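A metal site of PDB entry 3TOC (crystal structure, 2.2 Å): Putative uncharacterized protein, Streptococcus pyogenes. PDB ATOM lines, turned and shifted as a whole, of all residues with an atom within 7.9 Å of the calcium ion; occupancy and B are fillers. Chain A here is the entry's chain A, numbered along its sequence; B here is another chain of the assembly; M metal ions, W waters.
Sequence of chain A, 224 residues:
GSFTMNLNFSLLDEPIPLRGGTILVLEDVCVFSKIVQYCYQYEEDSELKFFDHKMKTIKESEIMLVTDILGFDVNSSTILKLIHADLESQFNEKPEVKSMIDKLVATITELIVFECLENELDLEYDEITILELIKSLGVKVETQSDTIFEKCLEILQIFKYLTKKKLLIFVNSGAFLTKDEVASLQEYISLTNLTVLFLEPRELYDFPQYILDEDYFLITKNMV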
ATOM      1  N   VAL A  74      10.807  -3.386  17.870  1.00  0.00           N
ATOM      2  CA  VAL A  74      12.246  -3.215  18.045  1.00  0.00           C
ATOM      3  C   VAL A  74      12.862  -4.524  18.508  1.00  0.00           C
ATOM      4  O   VAL A  74      14.063  -4.618  18.699  1.00  0.00           O
ATOM      5  CB  VAL A  74      12.589  -2.094  19.056  1.00  0.00           C
ATOM      6  CG1 VAL A  74      12.248  -0.714  18.484  1.00  0.00           C
ATOM      7  CG2 VAL A  74      11.885  -2.321  20.403  1.00  0.00           C
ATOM      8  N   VAL A 141      14.439  -5.704  24.265  1.00  0.00           N
ATOM      9  CA  VAL A 141      14.125  -4.342  24.645  1.00  0.00           C
ATOM     10  C   VAL A 141      12.796  -4.365  25.381  1.00  0.00           C
ATOM     11  O   VAL A 141      11.853  -4.994  24.913  1.00  0.00           O
ATOM     12  CB  VAL A 141      14.022  -3.462  23.399  1.00  0.00           C
ATOM     13  CG1 VAL A 141      13.796  -1.998  23.795  1.00  0.00           C
ATOM     14  CG2 VAL A 141      15.270  -3.627  22.542  1.00  0.00           C
ATOM     15  N   GLU A 142      12.695  -3.704  26.523  1.00  0.00           N
ATOM     16  CA  GLU A 142      11.388  -3.571  27.169  1.00  0.00           C
ATOM     17  C   GLU A 142      10.590  -2.447  26.501  1.00  0.00           C
ATOM     18  O   GLU A 142      11.144  -1.393  26.182  1.00  0.00           O
ATOM     19  CB  GLU A 142      11.512  -3.388  28.692  1.00  0.00           C
ATOM     20  CG  GLU A 142      11.082  -2.031  29.213  1.00  0.00           C
ATOM     21  CD  GLU A 142       9.566  -1.838  29.228  1.00  0.00           C
ATOM     22  OE1 GLU A 142       9.113  -0.735  28.922  1.00  0.00           O
ATOM     23  OE2 GLU A 142       8.831  -2.789  29.571  1.00  0.00           O
ATOM     24  N   THR A 143       9.303  -2.685  26.240  1.00  0.00           N
ATOM     25  CA  THR A 143       8.485  -1.727  25.490  1.00  0.00           C
ATOM     26  C   THR A 143       7.072  -1.611  26.041  1.00  0.00           C
ATOM     27  O   THR A 143       6.354  -0.659  25.746  1.00  0.00           O
ATOM     28  CB  THR A 143       8.373  -2.115  24.020  1.00  0.00           C
ATOM     29  OG1 THR A 143       7.842  -3.446  23.935  1.00  0.00           O
ATOM     30  CG2 THR A 143       9.728  -2.078  23.327  1.00  0.00           C
ATOM     31  N   GLN A 144       6.657  -2.597  26.833  1.00  0.00           N
ATOM     32  CA  GLN A 144       5.301  -2.636  27.351  1.00  0.00           C
ATOM     33  C   GLN A 144       4.867  -1.312  28.018  1.00  0.00           C
ATOM     34  O   GLN A 144       3.704  -0.912  27.909  1.00  0.00           O
ATOM     35  CB  GLN A 144       5.147  -3.798  28.333  1.00  0.00           C
ATOM     36  CG  GLN A 144       3.728  -4.322  28.475  1.00  0.00           C
ATOM     37  CD  GLN A 144       3.635  -5.518  29.419  1.00  0.00           C
ATOM     38  OE1 GLN A 144       4.532  -5.764  30.215  1.00  0.00           O
ATOM     39  NE2 GLN A 144       2.537  -6.266  29.324  1.00  0.00           N
ATOM     40  N   SER A 145       5.782  -0.644  28.685  1.00  0.00           N
ATOM     41  CA  SER A 145       5.428   0.533  29.471  1.00  0.00           C
ATOM     42  C   SER A 145       5.753   1.859  28.763  1.00  0.00           C
ATOM     43  O   SER A 145       5.488   2.942  29.281  1.00  0.00           O
ATOM     44  CB  SER A 145       6.156   0.484  30.817  1.00  0.00           C
ATOM     45  OG  SER A 145       7.561   0.576  30.649  1.00  0.00           O
ATOM     46  N   ASP A 146       6.334   1.751  27.583  1.00  0.00           N
ATOM     47  CA  ASP A 146       6.876   2.915  26.912  1.00  0.00           C
ATOM     48  C   ASP A 146       5.939   4.113  26.846  1.00  0.00           C
ATOM     49  O   ASP A 146       4.739   3.965  26.641  1.00  0.00           O
ATOM     50  CB  ASP A 146       7.351   2.533  25.518  1.00  0.00           C
ATOM     51  CG  ASP A 146       8.623   1.716  25.567  1.00  0.00           C
ATOM     52  OD1 ASP A 146       9.136   1.609  26.684  1.00  0.00           O
ATOM     53  OD2 ASP A 146       9.108   1.226  24.538  1.00  0.00           O
ATOM     54  N   THR A 147       6.496   5.291  27.053  1.00  0.00           N
ATOM     55  CA  THR A 147       5.851   6.496  26.617  1.00  0.00           C
ATOM     56  C   THR A 147       6.291   6.611  25.164  1.00  0.00           C
ATOM     57  O   THR A 147       7.240   5.944  24.753  1.00  0.00           O
ATOM     58  CB  THR A 147       6.384   7.703  27.368  1.00  0.00           C
ATOM     59  OG1 THR A 147       7.770   7.881  27.034  1.00  0.00           O
ATOM     60  CG2 THR A 147       6.252   7.480  28.863  1.00  0.00           C
ATOM     61  N   GLU A 150       9.975   7.592  24.962  1.00  0.00           N
ATOM     62  CA  GLU A 150      10.882   6.496  25.286  1.00  0.00           C
ATOM     63  C   GLU A 150      11.051   5.600  24.056  1.00  0.00           C
ATOM     64  O   GLU A 150      12.165   5.189  23.711  1.00  0.00           O
ATOM     65  CB  GLU A 150      10.368   5.694  26.479  1.00  0.00           C
ATOM     66  CG  GLU A 150      10.716   6.306  27.832  1.00  0.00           C
ATOM     67  CD  GLU A 150       9.829   5.766  28.951  1.00  0.00           C
ATOM     68  OE1 GLU A 150       9.156   4.748  28.748  1.00  0.00           O
ATOM     69  OE2 GLU A 150       9.797   6.392  30.035  1.00  0.00           O
ATOM     70  N   LYS A 151       9.947   5.330  23.378  1.00  0.00           N
ATOM     71  CA  LYS A 151       9.960   4.397  22.256  1.00  0.00           C
ATOM     72  C   LYS A 151      10.725   5.005  21.081  1.00  0.00           C
ATOM     73  O   LYS A 151      11.413   4.298  20.346  1.00  0.00           O
ATOM     74  CB  LYS A 151       8.516   3.988  21.877  1.00  0.00           C
ATOM     75  CG  LYS A 151       8.398   2.956  20.755  1.00  0.00           C
ATOM     76  CD  LYS A 151       9.018   1.653  21.151  1.00  0.00           C
ATOM     77  CE  LYS A 151       9.095   0.720  19.978  1.00  0.00           C
ATOM     78  NZ  LYS A 151       7.740   0.312  19.586  1.00  0.00           N
ATOM     79  N   GLU A 154      14.298   4.292  21.746  1.00  0.00           N
ATOM     80  CA  GLU A 154      14.614   2.886  21.455  1.00  0.00           C
ATOM     81  C   GLU A 154      14.739   2.584  19.970  1.00  0.00           C
ATOM     82  O   GLU A 154      15.565   1.776  19.570  1.00  0.00           O
ATOM     83  CB  GLU A 154      13.590   1.947  22.063  1.00  0.00           C
ATOM     84  CG  GLU A 154      13.729   1.821  23.552  1.00  0.00           C
ATOM     85  CD  GLU A 154      12.433   1.440  24.215  1.00  0.00           C
ATOM     86  OE1 GLU A 154      12.441   1.335  25.453  1.00  0.00           O
ATOM     87  OE2 GLU A 154      11.403   1.266  23.510  1.00  0.00           O
ATOM     88  N   LEU B 121      20.207   0.656  25.635  1.00  0.00           N
ATOM     89  CA  LEU B 121      18.834   0.188  25.537  1.00  0.00           C
ATOM     90  C   LEU B 121      18.253  -0.180  26.892  1.00  0.00           C
ATOM     91  O   LEU B 121      18.913  -0.776  27.737  1.00  0.00           O
ATOM     92  CB  LEU B 121      18.761  -1.041  24.644  1.00  0.00           C
ATOM     93  CG  LEU B 121      18.903  -0.822  23.158  1.00  0.00           C
ATOM     94  CD1 LEU B 121      19.203  -2.140  22.491  1.00  0.00           C
ATOM     95  CD2 LEU B 121      17.609  -0.220  22.637  1.00  0.00           C
ATOM     96  N   ASP B 122      16.987   0.150  27.050  1.00  0.00           N
ATOM     97  CA  ASP B 122      16.177  -0.353  28.140  1.00  0.00           C
ATOM     98  C   ASP B 122      15.879  -1.838  27.910  1.00  0.00           C
ATOM     99  O   ASP B 122      14.936  -2.205  27.190  1.00  0.00           O
ATOM    100  CB  ASP B 122      14.871   0.428  28.204  1.00  0.00           C
ATOM    101  CG  ASP B 122      14.076   0.073  29.409  1.00  0.00           C
ATOM    102  OD1 ASP B 122      12.887   0.453  29.499  1.00  0.00           O
ATOM    103  OD2 ASP B 122      14.644  -0.591  30.288  1.00  0.00           O
ATOM    104  N   LEU B 123      16.693  -2.693  28.529  1.00  0.00           N
ATOM    105  CA  LEU B 123      16.603  -4.144  28.328  1.00  0.00           C
ATOM    106  C   LEU B 123      15.930  -4.839  29.511  1.00  0.00           C
ATOM    107  O   LEU B 123      16.197  -4.531  30.666  1.00  0.00           O
ATOM    108  CB  LEU B 123      17.997  -4.740  28.103  1.00  0.00           C
ATOM    109  CG  LEU B 123      18.655  -4.248  26.818  1.00  0.00           C
ATOM    110  CD1 LEU B 123      20.081  -4.727  26.774  1.00  0.00           C
ATOM    111  CD2 LEU B 123      17.894  -4.761  25.617  1.00  0.00           C
ATOM    112  N   GLU B 124      15.049  -5.769  29.201  1.00  0.00           N
ATOM    113  CA  GLU B 124      14.511  -6.689  30.192  1.00  0.00           C
ATOM    114  C   GLU B 124      14.949  -8.111  29.845  1.00  0.00           C
ATOM    115  O   GLU B 124      15.678  -8.327  28.864  1.00  0.00           O
ATOM    116  CB  GLU B 124      12.990  -6.599  30.228  1.00  0.00           C
ATOM    117  CG  GLU B 124      12.288  -7.061  28.958  1.00  0.00           C
ATOM    118  CD  GLU B 124      10.774  -6.966  29.088  1.00  0.00           C
ATOM    119  OE1 GLU B 124      10.295  -6.543  30.161  1.00  0.00           O
ATOM    120  OE2 GLU B 124      10.069  -7.301  28.111  1.00  0.00           O
HETATM  121 CA    CA M   1      11.259   0.754  27.516  1.00  0.00          CA
HETATM  122  O   HOH W   1      12.170   3.323  28.052  1.00  0.00           O
HETATM  123  O   HOH W   2       9.758   2.238  29.415  1.00  0.00           O
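The side-chain carboxylate of Glu 142 is in hydrogen-bond range of the side-chain hydroxyl of Ser 145, at 2.7 Å.
Of the 15 residues printed, 4 come within 4 Å of the calcium ion.
The calcium ion is bound by the side-chain carboxylate of Asp 146 (2.4 Å), the side-chain carboxylate of Glu 154 (2.4 Å), the backbone carbonyl oxygen of Glu 142 (2.5 Å), the side-chain carboxylate of Asp 122 of chain B (2.6 Å), water W1 (2.8 Å) and water W2 (2.8 Å).
Slightly farther from the calcium ion lies the side-chain carboxylate (OE1) of Glu 142 (3.0 Å).
Water W2 lies within hydrogen-bond range of OE1 of Glu 150, OG of Ser 145 and OE1 of Glu 142.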
